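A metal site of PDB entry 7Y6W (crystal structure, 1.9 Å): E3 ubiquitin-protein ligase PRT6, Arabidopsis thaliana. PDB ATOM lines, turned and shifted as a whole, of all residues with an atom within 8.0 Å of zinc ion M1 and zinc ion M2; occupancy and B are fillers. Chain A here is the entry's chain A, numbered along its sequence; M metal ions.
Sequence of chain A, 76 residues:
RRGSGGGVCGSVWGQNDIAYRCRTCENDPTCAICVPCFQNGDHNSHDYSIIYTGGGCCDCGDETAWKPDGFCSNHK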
ATOM      1  N   GLY A   7      16.206 -12.578   5.449  1.00  0.00           N
ATOM      2  CA  GLY A   7      16.025 -11.820   6.683  1.00  0.00           C
ATOM      3  C   GLY A   7      16.436 -12.568   7.940  1.00  0.00           C
ATOM      4  O   GLY A   7      16.138 -13.759   8.089  1.00  0.00           O
ATOM      5  N   VAL A   8      17.156 -11.881   8.837  1.00  0.00           N
ATOM      6  CA  VAL A   8      17.397 -12.360  10.196  1.00  0.00           C
ATOM      7  C   VAL A   8      16.466 -11.551  11.099  1.00  0.00           C
ATOM      8  O   VAL A   8      16.177 -10.394  10.830  1.00  0.00           O
ATOM      9  CB  VAL A   8      18.869 -12.209  10.653  1.00  0.00           C
ATOM     10  CG1 VAL A   8      18.990 -12.510  12.135  1.00  0.00           C
ATOM     11  CG2 VAL A   8      19.769 -13.124   9.850  1.00  0.00           C
ATOM     12  N   CYS A   9      15.997 -12.179  12.186  1.00  0.00           N
ATOM     13  CA  CYS A   9      15.059 -11.504  13.074  1.00  0.00           C
ATOM     14  C   CYS A   9      15.733 -10.332  13.788  1.00  0.00           C
ATOM     15  O   CYS A   9      15.239  -9.206  13.773  1.00  0.00           O
ATOM     16  CB  CYS A   9      14.486 -12.463  14.107  1.00  0.00           C
ATOM     17  SG  CYS A   9      13.433 -11.602  15.326  1.00  0.00           S
ATOM     18  N   GLY A  10      16.834 -10.612  14.463  1.00  0.00           N
ATOM     19  CA  GLY A  10      17.633  -9.598  15.126  1.00  0.00           C
ATOM     20  C   GLY A  10      16.980  -8.878  16.290  1.00  0.00           C
ATOM     21  O   GLY A  10      17.624  -7.983  16.849  1.00  0.00           O
ATOM     22  N   SER A  11      15.747  -9.233  16.667  1.00  0.00           N
ATOM     23  CA  SER A  11      15.077  -8.560  17.777  1.00  0.00           C
ATOM     24  C   SER A  11      15.923  -8.598  19.042  1.00  0.00           C
ATOM     25  O   SER A  11      16.540  -9.621  19.345  1.00  0.00           O
ATOM     26  CB  SER A  11      13.724  -9.214  18.048  1.00  0.00           C
ATOM     27  OG  SER A  11      13.415  -9.178  19.428  1.00  0.00           O
ATOM     28  N   VAL A  12      15.906  -7.517  19.808  1.00  0.00           N
ATOM     29  CA  VAL A  12      16.862  -7.348  20.891  1.00  0.00           C
ATOM     30  C   VAL A  12      16.182  -7.481  22.242  1.00  0.00           C
ATOM     31  O   VAL A  12      15.092  -6.946  22.473  1.00  0.00           O
ATOM     32  CB  VAL A  12      17.603  -6.005  20.792  1.00  0.00           C
ATOM     33  CG1 VAL A  12      18.496  -5.791  22.017  1.00  0.00           C
ATOM     34  CG2 VAL A  12      18.444  -5.961  19.542  1.00  0.00           C
ATOM     35  N   TRP A  13      16.865  -8.150  23.165  1.00  0.00           N
ATOM     36  CA  TRP A  13      16.369  -8.358  24.515  1.00  0.00           C
ATOM     37  C   TRP A  13      17.122  -7.465  25.485  1.00  0.00           C
ATOM     38  O   TRP A  13      18.325  -7.240  25.336  1.00  0.00           O
ATOM     39  CB  TRP A  13      16.520  -9.808  24.972  1.00  0.00           C
ATOM     40  CG  TRP A  13      15.809 -10.743  24.104  1.00  0.00           C
ATOM     41  CD1 TRP A  13      14.500 -10.692  23.769  1.00  0.00           C
ATOM     42  CD2 TRP A  13      16.369 -11.855  23.431  1.00  0.00           C
ATOM     43  NE1 TRP A  13      14.201 -11.730  22.930  1.00  0.00           N
ATOM     44  CE2 TRP A  13      15.334 -12.449  22.696  1.00  0.00           C
ATOM     45  CE3 TRP A  13      17.648 -12.428  23.391  1.00  0.00           C
ATOM     46  CZ2 TRP A  13      15.533 -13.577  21.913  1.00  0.00           C
ATOM     47  CZ3 TRP A  13      17.849 -13.550  22.624  1.00  0.00           C
ATOM     48  CH2 TRP A  13      16.791 -14.116  21.885  1.00  0.00           C
ATOM     49  N   ALA A  32      19.357 -18.433  21.100  1.00  0.00           N
ATOM     50  CA  ALA A  32      17.990 -18.316  21.589  1.00  0.00           C
ATOM     51  C   ALA A  32      17.165 -17.624  20.522  1.00  0.00           C
ATOM     52  O   ALA A  32      17.710 -16.953  19.637  1.00  0.00           O
ATOM     53  CB  ALA A  32      17.920 -17.537  22.901  1.00  0.00           C
ATOM     54  N   ILE A  33      15.844 -17.794  20.593  1.00  0.00           N
ATOM     55  CA  ILE A  33      14.957 -17.067  19.684  1.00  0.00           C
ATOM     56  C   ILE A  33      13.827 -16.390  20.452  1.00  0.00           C
ATOM     57  O   ILE A  33      13.414 -16.869  21.513  1.00  0.00           O
ATOM     58  CB  ILE A  33      14.381 -17.987  18.590  1.00  0.00           C
ATOM     59  CG1 ILE A  33      13.670 -19.189  19.198  1.00  0.00           C
ATOM     60  CG2 ILE A  33      15.488 -18.496  17.670  1.00  0.00           C
ATOM     61  CD1 ILE A  33      12.867 -19.967  18.199  1.00  0.00           C
ATOM     62  N   CYS A  34      13.316 -15.302  19.899  1.00  0.00           N
ATOM     63  CA  CYS A  34      12.274 -14.548  20.582  1.00  0.00           C
ATOM     64  C   CYS A  34      10.976 -15.339  20.594  1.00  0.00           C
ATOM     65  O   CYS A  34      10.766 -16.287  19.820  1.00  0.00           O
ATOM     66  CB  CYS A  34      12.097 -13.157  19.933  1.00  0.00           C
ATOM     67  SG  CYS A  34      11.436 -13.191  18.311  1.00  0.00           S
ATOM     68  N   VAL A  35      10.105 -14.990  21.552  1.00  0.00           N
ATOM     69  CA  VAL A  35       8.845 -15.724  21.707  1.00  0.00           C
ATOM     70  C   VAL A  35       8.067 -15.728  20.398  1.00  0.00           C
ATOM     71  O   VAL A  35       7.499 -16.787  20.050  1.00  0.00           O
ATOM     72  CB  VAL A  35       8.036 -15.170  22.879  1.00  0.00           C
ATOM     73  CG1 VAL A  35       6.602 -15.755  22.854  1.00  0.00           C
ATOM     74  CG2 VAL A  35       8.712 -15.455  24.172  1.00  0.00           C
ATOM     75  N   PRO A  36       7.915 -14.623  19.693  1.00  0.00           N
ATOM     76  CA  PRO A  36       7.161 -14.666  18.429  1.00  0.00           C
ATOM     77  C   PRO A  36       7.758 -15.618  17.404  1.00  0.00           C
ATOM     78  O   PRO A  36       7.015 -16.322  16.701  1.00  0.00           O
ATOM     79  CB  PRO A  36       7.219 -13.218  17.911  1.00  0.00           C
ATOM     80  CG  PRO A  36       7.649 -12.388  19.061  1.00  0.00           C
ATOM     81  CD  PRO A  36       8.411 -13.265  20.000  1.00  0.00           C
ATOM     82  N   CYS A  37       9.075 -15.646  17.275  1.00  0.00           N
ATOM     83  CA  CYS A  37       9.676 -16.573  16.314  1.00  0.00           C
ATOM     84  C   CYS A  37       9.465 -18.012  16.762  1.00  0.00           C
ATOM     85  O   CYS A  37       9.239 -18.916  15.947  1.00  0.00           O
ATOM     86  CB  CYS A  37      11.177 -16.261  16.169  1.00  0.00           C
ATOM     87  SG  CYS A  37      11.604 -14.596  15.282  1.00  0.00           S
ATOM     88  N   PHE A  38       9.519 -18.262  18.066  1.00  0.00           N
ATOM     89  CA  PHE A  38       9.254 -19.601  18.546  1.00  0.00           C
ATOM     90  C   PHE A  38       7.830 -20.002  18.187  1.00  0.00           C
ATOM     91  O   PHE A  38       7.612 -21.098  17.652  1.00  0.00           O
ATOM     92  CB  PHE A  38       9.498 -19.704  20.067  1.00  0.00           C
ATOM     93  CG  PHE A  38       9.266 -21.098  20.629  1.00  0.00           C
ATOM     94  CD1 PHE A  38      10.264 -22.027  20.660  1.00  0.00           C
ATOM     95  CD2 PHE A  38       8.016 -21.468  21.069  1.00  0.00           C
ATOM     96  CE1 PHE A  38      10.056 -23.297  21.135  1.00  0.00           C
ATOM     97  CE2 PHE A  38       7.787 -22.726  21.564  1.00  0.00           C
ATOM     98  CZ  PHE A  38       8.814 -23.643  21.601  1.00  0.00           C
ATOM     99  N   ASN A  40       5.855 -19.052  15.859  1.00  0.00           N
ATOM    100  CA  ASN A  40       5.615 -19.142  14.428  1.00  0.00           C
ATOM    101  C   ASN A  40       6.530 -20.162  13.747  1.00  0.00           C
ATOM    102  O   ASN A  40       6.578 -20.216  12.514  1.00  0.00           O
ATOM    103  CB  ASN A  40       5.787 -17.751  13.795  1.00  0.00           C
ATOM    104  CG  ASN A  40       4.710 -16.793  14.230  1.00  0.00           C
ATOM    105  OD1 ASN A  40       3.545 -17.165  14.316  1.00  0.00           O
ATOM    106  ND2 ASN A  40       5.083 -15.557  14.512  1.00  0.00           N
ATOM    107  N   GLY A  41       7.226 -20.975  14.539  1.00  0.00           N
ATOM    108  CA  GLY A  41       7.952 -22.127  14.046  1.00  0.00           C
ATOM    109  C   GLY A  41       7.340 -23.437  14.517  1.00  0.00           C
ATOM    110  O   GLY A  41       6.246 -23.497  15.079  1.00  0.00           O
ATOM    111  N   CYS A  57      20.248 -11.007  21.277  1.00  0.00           N
ATOM    112  CA  CYS A  57      19.367 -10.844  20.131  1.00  0.00           C
ATOM    113  C   CYS A  57      18.956 -12.200  19.582  1.00  0.00           C
ATOM    114  O   CYS A  57      19.683 -13.189  19.684  1.00  0.00           O
ATOM    115  CB  CYS A  57      20.035 -10.002  19.041  1.00  0.00           C
ATOM    116  SG  CYS A  57      21.542 -10.786  18.324  1.00  0.00           S
ATOM    117  N   CYS A  58      17.773 -12.229  18.972  1.00  0.00           N
ATOM    118  CA  CYS A  58      17.188 -13.457  18.456  1.00  0.00           C
ATOM    119  C   CYS A  58      17.982 -14.005  17.277  1.00  0.00           C
ATOM    120  O   CYS A  58      18.414 -13.259  16.388  1.00  0.00           O
ATOM    121  CB  CYS A  58      15.734 -13.201  18.048  1.00  0.00           C
ATOM    122  SG  CYS A  58      14.855 -14.458  17.219  1.00  0.00           S
ATOM    123  N   ASP A  59      18.170 -15.323  17.256  1.00  0.00           N
ATOM    124  CA  ASP A  59      18.952 -15.981  16.233  1.00  0.00           C
ATOM    125  C   ASP A  59      18.125 -16.551  15.071  1.00  0.00           C
ATOM    126  O   ASP A  59      18.701 -17.135  14.156  1.00  0.00           O
ATOM    127  CB  ASP A  59      19.780 -17.105  16.875  1.00  0.00           C
ATOM    128  CG  ASP A  59      20.809 -16.570  17.870  1.00  0.00           C
ATOM    129  OD1 ASP A  59      21.612 -15.677  17.511  1.00  0.00           O
ATOM    130  OD2 ASP A  59      20.819 -17.039  19.034  1.00  0.00           O
ATOM    131  N   CYS A  60      16.802 -16.389  15.097  1.00  0.00           N
ATOM    132  CA  CYS A  60      15.953 -16.903  14.033  1.00  0.00           C
ATOM    133  C   CYS A  60      16.365 -16.285  12.704  1.00  0.00           C
ATOM    134  O   CYS A  60      16.503 -15.070  12.592  1.00  0.00           O
ATOM    135  CB  CYS A  60      14.490 -16.603  14.324  1.00  0.00           C
ATOM    136  SG  CYS A  60      13.407 -17.354  13.143  1.00  0.00           S
ATOM    137  N   GLY A  61      16.545 -17.133  11.687  1.00  0.00           N
ATOM    138  CA  GLY A  61      16.980 -16.675  10.383  1.00  0.00           C
ATOM    139  C   GLY A  61      18.461 -16.788  10.142  1.00  0.00           C
ATOM    140  O   GLY A  61      18.889 -16.763   8.986  1.00  0.00           O
ATOM    141  N   ASP A  62      19.258 -16.932  11.198  1.00  0.00           N
ATOM    142  CA  ASP A  62      20.713 -16.940  11.121  1.00  0.00           C
ATOM    143  C   ASP A  62      21.195 -18.377  11.173  1.00  0.00           C
ATOM    144  O   ASP A  62      21.277 -18.966  12.243  1.00  0.00           O
ATOM    145  CB  ASP A  62      21.298 -16.128  12.263  1.00  0.00           C
ATOM    146  CG  ASP A  62      22.821 -16.128  12.260  1.00  0.00           C
ATOM    147  OD1 ASP A  62      23.446 -16.741  11.347  1.00  0.00           O
ATOM    148  OD2 ASP A  62      23.420 -15.510  13.155  1.00  0.00           O
ATOM    149  N   TRP A  66      21.444 -21.109  14.350  1.00  0.00           N
ATOM    150  CA  TRP A  66      20.167 -21.776  14.573  1.00  0.00           C
ATOM    151  C   TRP A  66      19.946 -22.666  13.372  1.00  0.00           C
ATOM    152  O   TRP A  66      20.207 -22.247  12.244  1.00  0.00           O
ATOM    153  CB  TRP A  66      19.044 -20.748  14.721  1.00  0.00           C
ATOM    154  CG  TRP A  66      17.830 -21.224  15.412  1.00  0.00           C
ATOM    155  CD1 TRP A  66      16.682 -21.663  14.821  1.00  0.00           C
ATOM    156  CD2 TRP A  66      17.621 -21.314  16.823  1.00  0.00           C
ATOM    157  NE1 TRP A  66      15.767 -21.990  15.783  1.00  0.00           N
ATOM    158  CE2 TRP A  66      16.328 -21.826  17.017  1.00  0.00           C
ATOM    159  CE3 TRP A  66      18.403 -21.016  17.941  1.00  0.00           C
ATOM    160  CZ2 TRP A  66      15.785 -22.021  18.271  1.00  0.00           C
ATOM    161  CZ3 TRP A  66      17.879 -21.223  19.174  1.00  0.00           C
ATOM    162  CH2 TRP A  66      16.570 -21.702  19.343  1.00  0.00           C
ATOM    163  N   GLY A  70      14.462 -24.866  12.213  1.00  0.00           N
ATOM    164  CA  GLY A  70      13.937 -24.203  13.381  1.00  0.00           C
ATOM    165  C   GLY A  70      13.516 -22.779  13.162  1.00  0.00           C
ATOM    166  O   GLY A  70      13.048 -22.136  14.097  1.00  0.00           O
ATOM    167  N   PHE A  71      13.645 -22.277  11.940  1.00  0.00           N
ATOM    168  CA  PHE A  71      13.270 -20.901  11.651  1.00  0.00           C
ATOM    169  C   PHE A  71      11.761 -20.758  11.639  1.00  0.00           C
ATOM    170  O   PHE A  71      11.019 -21.687  11.350  1.00  0.00           O
ATOM    171  CB  PHE A  71      13.823 -20.462  10.304  1.00  0.00           C
ATOM    172  CG  PHE A  71      15.315 -20.348  10.258  1.00  0.00           C
ATOM    173  CD1 PHE A  71      15.952 -20.136   9.034  1.00  0.00           C
ATOM    174  CD2 PHE A  71      16.082 -20.472  11.401  1.00  0.00           C
ATOM    175  CE1 PHE A  71      17.323 -20.046   8.967  1.00  0.00           C
ATOM    176  CE2 PHE A  71      17.439 -20.341  11.349  1.00  0.00           C
ATOM    177  CZ  PHE A  71      18.064 -20.127  10.151  1.00  0.00           C
ATOM    178  N   CYS A  72      11.298 -19.539  11.922  1.00  0.00           N
ATOM    179  CA  CYS A  72       9.885 -19.230  11.857  1.00  0.00           C
ATOM    180  C   CYS A  72       9.491 -18.887  10.418  1.00  0.00           C
ATOM    181  O   CYS A  72      10.332 -18.748   9.529  1.00  0.00           O
ATOM    182  CB  CYS A  72       9.567 -18.067  12.801  1.00  0.00           C
ATOM    183  SG  CYS A  72       9.904 -16.363  12.184  1.00  0.00           S
ATOM    184  N   SER A  73       8.168 -18.785  10.201  1.00  0.00           N
ATOM    185  CA  SER A  73       7.582 -18.547   8.884  1.00  0.00           C
ATOM    186  C   SER A  73       8.035 -17.255   8.230  1.00  0.00           C
ATOM    187  O   SER A  73       7.943 -17.118   6.999  1.00  0.00           O
ATOM    188  CB  SER A  73       6.059 -18.519   9.012  1.00  0.00           C
ATOM    189  OG  SER A  73       5.658 -17.382   9.741  1.00  0.00           O
ATOM    190  N   ASN A  74       8.522 -16.300   9.016  1.00  0.00           N
ATOM    191  CA  ASN A  74       8.872 -14.979   8.532  1.00  0.00           C
ATOM    192  C   ASN A  74      10.360 -14.792   8.282  1.00  0.00           C
ATOM    193  O   ASN A  74      10.732 -13.768   7.709  1.00  0.00           O
ATOM    194  CB  ASN A  74       8.380 -13.912   9.518  1.00  0.00           C
ATOM    195  CG  ASN A  74       6.861 -13.928   9.713  1.00  0.00           C
ATOM    196  OD1 ASN A  74       6.104 -13.890   8.753  1.00  0.00           O
ATOM    197  ND2 ASN A  74       6.431 -13.995  10.973  1.00  0.00           N
ATOM    198  N   HIS A  75      11.213 -15.755   8.621  1.00  0.00           N
ATOM    199  CA  HIS A  75      12.658 -15.564   8.485  1.00  0.00           C
ATOM    200  C   HIS A  75      13.296 -16.681   7.685  1.00  0.00           C
ATOM    201  O   HIS A  75      14.429 -17.115   7.946  1.00  0.00           O
ATOM    202  CB  HIS A  75      13.291 -15.372   9.865  1.00  0.00           C
ATOM    203  CG  HIS A  75      12.749 -14.193  10.616  1.00  0.00           C
ATOM    204  ND1 HIS A  75      11.957 -14.306  11.735  1.00  0.00           N
ATOM    205  CD2 HIS A  75      12.844 -12.857  10.358  1.00  0.00           C
ATOM    206  CE1 HIS A  75      11.609 -13.105  12.155  1.00  0.00           C
ATOM    207  NE2 HIS A  75      12.137 -12.201  11.340  1.00  0.00           N
ATOM    208  N   LYS A  76      12.598 -17.154   6.663  1.00  0.00           N
ATOM    209  CA  LYS A  76      13.179 -18.108   5.733  1.00  0.00           C
ATOM    210  C   LYS A  76      13.376 -17.497   4.351  1.00  0.00           C
ATOM    211  O   LYS A  76      13.846 -18.191   3.442  1.00  0.00           O
ATOM    212  CB  LYS A  76      12.298 -19.320   5.614  1.00  0.00           C
ATOM    213  CG  LYS A  76      11.756 -19.837   6.898  1.00  0.00           C
ATOM    214  CD  LYS A  76      10.922 -21.044   6.612  1.00  0.00           C
ATOM    215  CE  LYS A  76      10.925 -21.935   7.788  1.00  0.00           C
ATOM    216  NZ  LYS A  76       9.816 -22.901   7.759  1.00  0.00           N
HETATM  217 ZN    ZN M   1      11.813 -15.744  13.088  1.00  0.00          ZN
HETATM  218 ZN    ZN M   2      12.972 -13.384  16.604  1.00  0.00          ZN
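The side-chain sulfur of Cys 9 sits close to the backbone NH of Ser 11 (3.6 Å). O of Cys 60 is in hydrogen-bond range of N of Cys 9. The backbone NH (N) of Asn 74 sits close to the side-chain sulfur (SG) of Cys 72. The backbone NH of Cys 58 lies within hydrogen-bond range of the backbone carbonyl oxygen of Ser 11 (2.9 Å). The side-chain sulfur of Cys 58 sits close to the backbone NH of Cys 60, at 3.5 Å.
Four residues have an atom within 4 Å of zinc ion M1: Cys 37, Cys 60, Cys 72 and His 75.
The nearest printed residue that does not touch zinc ion M2 is Cys 60 (4.2 Å).
Zinc ion M1 is bound by ND1 of His 75, SG of Cys 72, SG of Cys 60 and SG of Cys 37. Zinc ion M1 has four donor atoms within binding distance.
Zinc ion M2 is bound by the side-chain sulfur of Cys 9 (2.2 Å), the side-chain sulfur of Cys 58 (2.3 Å), the side-chain sulfur of Cys 37 (2.3 Å) and the side-chain sulfur of Cys 34 (2.3 Å).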
